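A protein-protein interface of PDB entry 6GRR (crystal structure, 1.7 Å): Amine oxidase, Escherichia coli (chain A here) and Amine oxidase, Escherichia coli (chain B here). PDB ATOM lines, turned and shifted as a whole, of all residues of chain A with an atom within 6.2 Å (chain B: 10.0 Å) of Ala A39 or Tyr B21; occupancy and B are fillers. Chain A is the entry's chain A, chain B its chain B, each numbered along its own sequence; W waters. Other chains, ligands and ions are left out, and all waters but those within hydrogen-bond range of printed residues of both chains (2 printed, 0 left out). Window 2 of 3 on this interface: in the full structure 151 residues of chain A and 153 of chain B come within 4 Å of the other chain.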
ATOM      1  N   LEU A  23     -29.956  15.200 -16.166  1.00  0.00           N
ATOM      2  CA  LEU A  23     -28.735  14.924 -15.392  1.00  0.00           C
ATOM      3  C   LEU A  23     -27.648  14.454 -16.324  1.00  0.00           C
ATOM      4  O   LEU A  23     -27.860  13.504 -17.131  1.00  0.00           O
ATOM      5  CB  LEU A  23     -28.981  13.841 -14.345  1.00  0.00           C
ATOM      6  CG  LEU A  23     -27.762  13.515 -13.425  1.00  0.00           C
ATOM      7  CD1 LEU A  23     -27.525  14.685 -12.499  1.00  0.00           C
ATOM      8  CD2 LEU A  23     -28.026  12.243 -12.625  1.00  0.00           C
ATOM      9  N   LYS A  34     -21.795  14.006 -11.187  1.00  0.00           N
ATOM     10  CA  LYS A  34     -23.197  14.265 -11.582  1.00  0.00           C
ATOM     11  C   LYS A  34     -23.446  15.765 -11.562  1.00  0.00           C
ATOM     12  O   LYS A  34     -23.063  16.466 -10.623  1.00  0.00           O
ATOM     13  CB  LYS A  34     -24.163  13.581 -10.650  1.00  0.00           C
ATOM     14  CG  LYS A  34     -24.061  12.075 -10.704  1.00  0.00           C
ATOM     15  CD  LYS A  34     -25.058  11.383  -9.801  1.00  0.00           C
ATOM     16  CE  LYS A  34     -24.473  10.965  -8.474  1.00  0.00           C
ATOM     17  NZ  LYS A  34     -25.337   9.917  -7.864  1.00  0.00           N
ATOM     18  N   VAL A  35     -24.079  16.274 -12.607  1.00  0.00           N
ATOM     19  CA  VAL A  35     -24.324  17.713 -12.690  1.00  0.00           C
ATOM     20  C   VAL A  35     -25.598  17.973 -13.504  1.00  0.00           C
ATOM     21  O   VAL A  35     -25.754  17.413 -14.602  1.00  0.00           O
ATOM     22  CB  VAL A  35     -23.102  18.509 -13.237  1.00  0.00           C
ATOM     23  CG1 VAL A  35     -22.690  18.098 -14.650  1.00  0.00           C
ATOM     24  CG2 VAL A  35     -23.359  20.023 -13.142  1.00  0.00           C
ATOM     25  N   LYS A  36     -26.500  18.755 -12.924  1.00  0.00           N
ATOM     26  CA  LYS A  36     -27.738  19.204 -13.599  1.00  0.00           C
ATOM     27  C   LYS A  36     -27.514  20.572 -14.256  1.00  0.00           C
ATOM     28  O   LYS A  36     -26.892  21.441 -13.665  1.00  0.00           O
ATOM     29  CB  LYS A  36     -28.875  19.319 -12.590  1.00  0.00           C
ATOM     30  CG  LYS A  36     -29.335  18.004 -11.984  1.00  0.00           C
ATOM     31  CD  LYS A  36     -30.388  18.195 -10.900  1.00  0.00           C
ATOM     32  CE  LYS A  36     -31.719  18.824 -11.382  1.00  0.00           C
ATOM     33  NZ  LYS A  36     -32.174  18.369 -12.735  1.00  0.00           N
ATOM     34  N   PRO A  37     -28.042  20.788 -15.479  1.00  0.00           N
ATOM     35  CA  PRO A  37     -28.016  22.144 -16.068  1.00  0.00           C
ATOM     36  C   PRO A  37     -28.695  23.159 -15.149  1.00  0.00           C
ATOM     37  O   PRO A  37     -29.709  22.854 -14.508  1.00  0.00           O
ATOM     38  CB  PRO A  37     -28.832  21.979 -17.368  1.00  0.00           C
ATOM     39  CG  PRO A  37     -28.723  20.527 -17.683  1.00  0.00           C
ATOM     40  CD  PRO A  37     -28.753  19.840 -16.347  1.00  0.00           C
ATOM     41  N   GLY A  38     -28.077  24.323 -15.011  1.00  0.00           N
ATOM     42  CA  GLY A  38     -28.617  25.373 -14.179  1.00  0.00           C
ATOM     43  C   GLY A  38     -28.311  25.231 -12.701  1.00  0.00           C
ATOM     44  O   GLY A  38     -28.519  26.183 -11.951  1.00  0.00           O
ATOM     45  N   ALA A  39     -27.817  24.076 -12.255  1.00  0.00           N
ATOM     46  CA  ALA A  39     -27.639  23.869 -10.804  1.00  0.00           C
ATOM     47  C   ALA A  39     -26.417  24.629 -10.329  1.00  0.00           C
ATOM     48  O   ALA A  39     -25.437  24.741 -11.050  1.00  0.00           O
ATOM     49  CB  ALA A  39     -27.498  22.396 -10.447  1.00  0.00           C
ATOM     50  N   GLN A  40     -26.491  25.153  -9.105  1.00  0.00           N
ATOM     51  CA  GLN A  40     -25.364  25.885  -8.525  1.00  0.00           C
ATOM     52  C   GLN A  40     -24.320  24.961  -7.903  1.00  0.00           C
ATOM     53  O   GLN A  40     -23.219  25.425  -7.548  1.00  0.00           O
ATOM     54  CB  GLN A  40     -25.876  26.865  -7.463  1.00  0.00           C
ATOM     55  CG  GLN A  40     -26.671  28.036  -8.021  1.00  0.00           C
ATOM     56  CD  GLN A  40     -27.328  28.887  -6.932  1.00  0.00           C
ATOM     57  OE1 GLN A  40     -26.900  28.906  -5.769  1.00  0.00           O
ATOM     58  NE2 GLN A  40     -28.376  29.594  -7.309  1.00  0.00           N
ATOM     59  N   THR A  41     -24.656  23.678  -7.782  1.00  0.00           N
ATOM     60  CA  THR A  41     -23.759  22.660  -7.245  1.00  0.00           C
ATOM     61  C   THR A  41     -23.715  21.419  -8.137  1.00  0.00           C
ATOM     62  O   THR A  41     -24.589  21.216  -8.987  1.00  0.00           O
ATOM     63  CB  THR A  41     -24.132  22.212  -5.822  1.00  0.00           C
ATOM     64  OG1 THR A  41     -25.309  21.397  -5.844  1.00  0.00           O
ATOM     65  CG2 THR A  41     -24.329  23.385  -4.870  1.00  0.00           C
ATOM     66  N   ALA A  42     -22.676  20.615  -7.923  1.00  0.00           N
ATOM     67  CA  ALA A  42     -22.488  19.311  -8.590  1.00  0.00           C
ATOM     68  C   ALA A  42     -22.145  18.260  -7.550  1.00  0.00           C
ATOM     69  O   ALA A  42     -21.975  18.587  -6.350  1.00  0.00           O
ATOM     70  CB  ALA A  42     -21.405  19.426  -9.617  1.00  0.00           C
ATOM     71  N   ILE A  43     -22.091  16.990  -7.965  1.00  0.00           N
ATOM     72  CA  ILE A  43     -21.635  15.918  -7.077  1.00  0.00           C
ATOM     73  C   ILE A  43     -20.386  15.301  -7.695  1.00  0.00           C
ATOM     74  O   ILE A  43     -20.387  14.946  -8.890  1.00  0.00           O
ATOM     75  CB  ILE A  43     -22.731  14.842  -6.890  1.00  0.00           C
ATOM     76  CG1 ILE A  43     -23.989  15.426  -6.260  1.00  0.00           C
ATOM     77  CG2 ILE A  43     -22.213  13.643  -6.087  1.00  0.00           C
ATOM     78  CD1 ILE A  43     -23.851  15.805  -4.786  1.00  0.00           C
ATOM     79  N   LEU A  51     -20.351  25.304  -7.683  1.00  0.00           N
ATOM     80  CA  LEU A  51     -19.852  25.708  -8.979  1.00  0.00           C
ATOM     81  C   LEU A  51     -19.790  27.244  -9.052  1.00  0.00           C
ATOM     82  O   LEU A  51     -20.663  27.913  -8.564  1.00  0.00           O
ATOM     83  CB  LEU A  51     -20.773  25.155 -10.076  1.00  0.00           C
ATOM     84  CG  LEU A  51     -20.860  23.638 -10.181  1.00  0.00           C
ATOM     85  CD1 LEU A  51     -21.914  23.278 -11.233  1.00  0.00           C
ATOM     86  CD2 LEU A  51     -19.508  23.041 -10.536  1.00  0.00           C
ATOM     87  N   VAL A  53     -19.812  28.719 -12.051  1.00  0.00           N
ATOM     88  CA  VAL A  53     -20.640  28.943 -13.237  1.00  0.00           C
ATOM     89  C   VAL A  53     -21.457  27.665 -13.499  1.00  0.00           C
ATOM     90  O   VAL A  53     -20.871  26.625 -13.781  1.00  0.00           O
ATOM     91  CB  VAL A  53     -19.766  29.273 -14.463  1.00  0.00           C
ATOM     92  CG1 VAL A  53     -20.640  29.481 -15.698  1.00  0.00           C
ATOM     93  CG2 VAL A  53     -18.912  30.517 -14.203  1.00  0.00           C
ATOM     94  N   PRO A  54     -22.793  27.735 -13.361  1.00  0.00           N
ATOM     95  CA  PRO A  54     -23.625  26.586 -13.697  1.00  0.00           C
ATOM     96  C   PRO A  54     -23.425  26.118 -15.145  1.00  0.00           C
ATOM     97  O   PRO A  54     -22.993  26.906 -16.008  1.00  0.00           O
ATOM     98  CB  PRO A  54     -25.039  27.107 -13.458  1.00  0.00           C
ATOM     99  CG  PRO A  54     -24.867  28.083 -12.331  1.00  0.00           C
ATOM    100  CD  PRO A  54     -23.571  28.772 -12.650  1.00  0.00           C
ATOM    101  N   VAL A  55     -23.680  24.829 -15.381  1.00  0.00           N
ATOM    102  CA  VAL A  55     -23.705  24.297 -16.727  1.00  0.00           C
ATOM    103  C   VAL A  55     -24.883  25.001 -17.402  1.00  0.00           C
ATOM    104  O   VAL A  55     -25.942  25.086 -16.804  1.00  0.00           O
ATOM    105  CB  VAL A  55     -23.971  22.786 -16.726  1.00  0.00           C
ATOM    106  CG1 VAL A  55     -24.208  22.257 -18.152  1.00  0.00           C
ATOM    107  CG2 VAL A  55     -22.833  22.035 -16.042  1.00  0.00           C
ATOM    108  N   GLN B  17     -32.206   2.591  -4.702  1.00  0.00           N
ATOM    109  CA  GLN B  17     -31.211   3.656  -4.504  1.00  0.00           C
ATOM    110  C   GLN B  17     -31.879   5.010  -4.642  1.00  0.00           C
ATOM    111  O   GLN B  17     -32.632   5.258  -5.587  1.00  0.00           O
ATOM    112  CB  GLN B  17     -30.044   3.575  -5.508  1.00  0.00           C
ATOM    113  CG  GLN B  17     -29.246   2.262  -5.526  1.00  0.00           C
ATOM    114  CD  GLN B  17     -28.354   2.012  -4.301  1.00  0.00           C
ATOM    115  OE1 GLN B  17     -27.956   2.934  -3.585  1.00  0.00           O
ATOM    116  NE2 GLN B  17     -28.047   0.736  -4.058  1.00  0.00           N
ATOM    117  N   TRP B  18     -31.607   5.887  -3.681  1.00  0.00           N
ATOM    118  CA  TRP B  18     -32.125   7.241  -3.697  1.00  0.00           C
ATOM    119  C   TRP B  18     -30.975   8.178  -3.942  1.00  0.00           C
ATOM    120  O   TRP B  18     -29.946   8.092  -3.249  1.00  0.00           O
ATOM    121  CB  TRP B  18     -32.780   7.569  -2.352  1.00  0.00           C
ATOM    122  CG  TRP B  18     -33.121   9.015  -2.170  1.00  0.00           C
ATOM    123  CD1 TRP B  18     -32.610   9.857  -1.225  1.00  0.00           C
ATOM    124  CD2 TRP B  18     -34.037   9.798  -2.947  1.00  0.00           C
ATOM    125  NE1 TRP B  18     -33.168  11.096  -1.347  1.00  0.00           N
ATOM    126  CE2 TRP B  18     -34.035  11.096  -2.404  1.00  0.00           C
ATOM    127  CE3 TRP B  18     -34.863   9.526  -4.048  1.00  0.00           C
ATOM    128  CZ2 TRP B  18     -34.820  12.117  -2.913  1.00  0.00           C
ATOM    129  CZ3 TRP B  18     -35.643  10.542  -4.553  1.00  0.00           C
ATOM    130  CH2 TRP B  18     -35.623  11.822  -3.988  1.00  0.00           C
ATOM    131  N   ASP B  19     -31.143   9.066  -4.917  1.00  0.00           N
ATOM    132  CA  ASP B  19     -30.180  10.119  -5.222  1.00  0.00           C
ATOM    133  C   ASP B  19     -30.803  11.472  -4.873  1.00  0.00           C
ATOM    134  O   ASP B  19     -31.662  12.014  -5.595  1.00  0.00           O
ATOM    135  CB  ASP B  19     -29.774  10.068  -6.698  1.00  0.00           C
ATOM    136  CG  ASP B  19     -28.667  11.058  -7.057  1.00  0.00           C
ATOM    137  OD1 ASP B  19     -28.482  12.099  -6.381  1.00  0.00           O
ATOM    138  OD2 ASP B  19     -27.974  10.811  -8.056  1.00  0.00           O
ATOM    139  N   ASP B  20     -30.315  12.047  -3.780  1.00  0.00           N
ATOM    140  CA  ASP B  20     -30.837  13.296  -3.258  1.00  0.00           C
ATOM    141  C   ASP B  20     -30.547  14.505  -4.146  1.00  0.00           C
ATOM    142  O   ASP B  20     -31.334  15.447  -4.198  1.00  0.00           O
ATOM    143  CB  ASP B  20     -30.271  13.540  -1.832  1.00  0.00           C
ATOM    144  CG  ASP B  20     -31.091  14.537  -1.059  1.00  0.00           C
ATOM    145  OD1 ASP B  20     -32.271  14.229  -0.743  1.00  0.00           O
ATOM    146  OD2 ASP B  20     -30.568  15.633  -0.790  1.00  0.00           O
ATOM    147  N   TYR B  21     -29.428  14.483  -4.846  1.00  0.00           N
ATOM    148  CA  TYR B  21     -29.075  15.574  -5.733  1.00  0.00           C
ATOM    149  C   TYR B  21     -29.996  15.564  -6.974  1.00  0.00           C
ATOM    150  O   TYR B  21     -30.506  16.597  -7.379  1.00  0.00           O
ATOM    151  CB  TYR B  21     -27.623  15.464  -6.186  1.00  0.00           C
ATOM    152  CG  TYR B  21     -27.184  16.464  -7.218  1.00  0.00           C
ATOM    153  CD1 TYR B  21     -26.981  17.802  -6.883  1.00  0.00           C
ATOM    154  CD2 TYR B  21     -26.981  16.087  -8.558  1.00  0.00           C
ATOM    155  CE1 TYR B  21     -26.542  18.707  -7.821  1.00  0.00           C
ATOM    156  CE2 TYR B  21     -26.529  16.986  -9.497  1.00  0.00           C
ATOM    157  CZ  TYR B  21     -26.329  18.311  -9.142  1.00  0.00           C
ATOM    158  OH  TYR B  21     -25.889  19.204 -10.080  1.00  0.00           O
ATOM    159  N   ALA B  22     -30.162  14.388  -7.553  1.00  0.00           N
ATOM    160  CA  ALA B  22     -30.995  14.224  -8.766  1.00  0.00           C
ATOM    161  C   ALA B  22     -32.480  14.125  -8.439  1.00  0.00           C
ATOM    162  O   ALA B  22     -33.288  14.224  -9.345  1.00  0.00           O
ATOM    163  CB  ALA B  22     -30.551  12.980  -9.536  1.00  0.00           C
ATOM    164  N   GLN B  23     -32.838  13.925  -7.160  1.00  0.00           N
ATOM    165  CA  GLN B  23     -34.208  13.645  -6.729  1.00  0.00           C
ATOM    166  C   GLN B  23     -34.770  12.444  -7.525  1.00  0.00           C
ATOM    167  O   GLN B  23     -35.859  12.504  -8.088  1.00  0.00           O
ATOM    168  CB  GLN B  23     -35.101  14.898  -6.833  1.00  0.00           C
ATOM    169  CG  GLN B  23     -34.688  16.020  -5.886  1.00  0.00           C
ATOM    170  CD  GLN B  23     -35.098  15.724  -4.470  1.00  0.00           C
ATOM    171  OE1 GLN B  23     -36.277  15.505  -4.208  1.00  0.00           O
ATOM    172  NE2 GLN B  23     -34.125  15.684  -3.542  1.00  0.00           N
ATOM    173  N   LEU B  24     -33.987  11.359  -7.525  1.00  0.00           N
ATOM    174  CA  LEU B  24     -34.201  10.222  -8.408  1.00  0.00           C
ATOM    175  C   LEU B  24     -34.038   8.919  -7.648  1.00  0.00           C
ATOM    176  O   LEU B  24     -32.990   8.688  -7.004  1.00  0.00           O
ATOM    177  CB  LEU B  24     -33.194  10.259  -9.565  1.00  0.00           C
ATOM    178  CG  LEU B  24     -33.298   9.133 -10.613  1.00  0.00           C
ATOM    179  CD1 LEU B  24     -34.576   9.293 -11.405  1.00  0.00           C
ATOM    180  CD2 LEU B  24     -32.098   9.123 -11.548  1.00  0.00           C
ATOM    181  N   PHE B  25     -35.055   8.064  -7.744  1.00  0.00           N
ATOM    182  CA  PHE B  25     -34.937   6.669  -7.353  1.00  0.00           C
ATOM    183  C   PHE B  25     -34.459   5.817  -8.529  1.00  0.00           C
ATOM    184  O   PHE B  25     -34.983   5.937  -9.645  1.00  0.00           O
ATOM    185  CB  PHE B  25     -36.272   6.100  -6.883  1.00  0.00           C
ATOM    186  CG  PHE B  25     -36.666   6.524  -5.491  1.00  0.00           C
ATOM    187  CD1 PHE B  25     -36.065   5.936  -4.385  1.00  0.00           C
ATOM    188  CD2 PHE B  25     -37.627   7.486  -5.294  1.00  0.00           C
ATOM    189  CE1 PHE B  25     -36.421   6.300  -3.092  1.00  0.00           C
ATOM    190  CE2 PHE B  25     -37.988   7.874  -4.000  1.00  0.00           C
ATOM    191  CZ  PHE B  25     -37.374   7.276  -2.902  1.00  0.00           C
ATOM    192  N   LYS B  37     -38.840   9.593 -10.466  1.00  0.00           N
ATOM    193  CA  LYS B  37     -38.753  10.795  -9.617  1.00  0.00           C
ATOM    194  C   LYS B  37     -40.047  10.991  -8.838  1.00  0.00           C
ATOM    195  O   LYS B  37     -41.137  10.798  -9.390  1.00  0.00           O
ATOM    196  CB  LYS B  37     -38.493  12.039 -10.465  1.00  0.00           C
ATOM    197  CG  LYS B  37     -37.178  12.029 -11.222  1.00  0.00           C
ATOM    198  CD  LYS B  37     -37.045  13.177 -12.208  1.00  0.00           C
ATOM    199  CE  LYS B  37     -37.107  14.550 -11.562  1.00  0.00           C
ATOM    200  NZ  LYS B  37     -36.113  14.690 -10.477  1.00  0.00           N
ATOM    201  N   PRO B  38     -39.947  11.383  -7.550  1.00  0.00           N
ATOM    202  CA  PRO B  38     -41.151  11.748  -6.788  1.00  0.00           C
ATOM    203  C   PRO B  38     -41.976  12.760  -7.551  1.00  0.00           C
ATOM    204  O   PRO B  38     -41.417  13.681  -8.161  1.00  0.00           O
ATOM    205  CB  PRO B  38     -40.597  12.401  -5.511  1.00  0.00           C
ATOM    206  CG  PRO B  38     -39.223  11.867  -5.370  1.00  0.00           C
ATOM    207  CD  PRO B  38     -38.720  11.527  -6.748  1.00  0.00           C
ATOM    208  N   MET B  58     -43.363  11.771  -1.942  1.00  0.00           N
ATOM    209  CA  MET B  58     -42.415  11.990  -0.856  1.00  0.00           C
ATOM    210  C   MET B  58     -43.131  12.822   0.205  1.00  0.00           C
ATOM    211  O   MET B  58     -43.886  13.737  -0.125  1.00  0.00           O
ATOM    212  CB  MET B  58     -41.163  12.703  -1.381  1.00  0.00           C
ATOM    213  CG  MET B  58     -39.979  12.691  -0.423  1.00  0.00           C
ATOM    214  SD  MET B  58     -39.273  11.053  -0.146  1.00  0.00           S
ATOM    215  CE  MET B  58     -38.036  10.947  -1.435  1.00  0.00           C
HETATM  216  O   HOH W   1     -32.508  15.619 -11.532  1.00  0.00           O
HETATM  217  O   HOH W   2     -25.827  12.264  -5.626  1.00  0.00           O
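OD2 of Asp B19 lies within salt-bridge range of NZ of Lys A34, at 2.8 Å.
The backbone NH (N) of Lys A36 lies within hydrogen-bond range of the side-chain hydroxyl (OH) of Tyr B21 (2.9 Å).
OH of Tyr B21 lies within hydrogen-bond range of O of Thr A41, at 2.6 Å.
Of the printed residues of chain B, Leu A23 touches Tyr B21 (3.9 Å).
Lys A36 touches just one residue of chain B: Tyr B21.
No residue of chain B comes within 4 Å of Gly A38.
Of the printed residues of chain B, Ala A39 touches Tyr B21 (3.6 Å).
Printed residues of chain B within 4 Å of Thr A41: Tyr B21.
Ala A42 touches just one residue of chain B: Tyr B21.
No residue of chain B comes within 4 Å of Pro A54.
Asp B20 touches none of the printed residues of chain A.
Tyr B21 touches eight residues of chain A.
Among the printed residues, pairs that only touch across the chains: Leu A23 with Tyr B21 (3.9 Å), Lys A34 with Tyr B21 (3.7 Å), Val A35 with Tyr B21 (3.4 Å), Ala A39 with Tyr B21 (3.6 Å), Ala A42 with Tyr B21 (3.7 Å) and Ile A43 with Tyr B21 (3.5 Å).
Of the 15 printed residues of chain A, 8 touch a printed residue of chain B.
Water W1 lies within hydrogen-bond range of O of Ala B22 (2.7 Å) and NZ of Lys A36 (3.0 Å).
Water W2 lies within hydrogen-bond range of the side-chain carboxylate (OD1) of Asp B19 (2.8 Å) and the side-chain amino group (NZ) of Lys A34 (3.3 Å).
OD1 of Asp B19 sits at hydrogen-bond distance from N of Ala B22 (3.1 Å).
The side-chain carboxylate (OD1) of Asp B19 lies within hydrogen-bond range of the backbone NH (N) of Tyr B21, 3.0 Å away.
The backbone NH (N) of Asp B19 lies within hydrogen-bond range of the backbone carbonyl oxygen (O) of Leu B24, 2.8 Å away.
The backbone carbonyl oxygen (O) of Ile A43 is in hydrogen-bond range of the backbone NH (N) of Lys A34 (2.9 Å).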
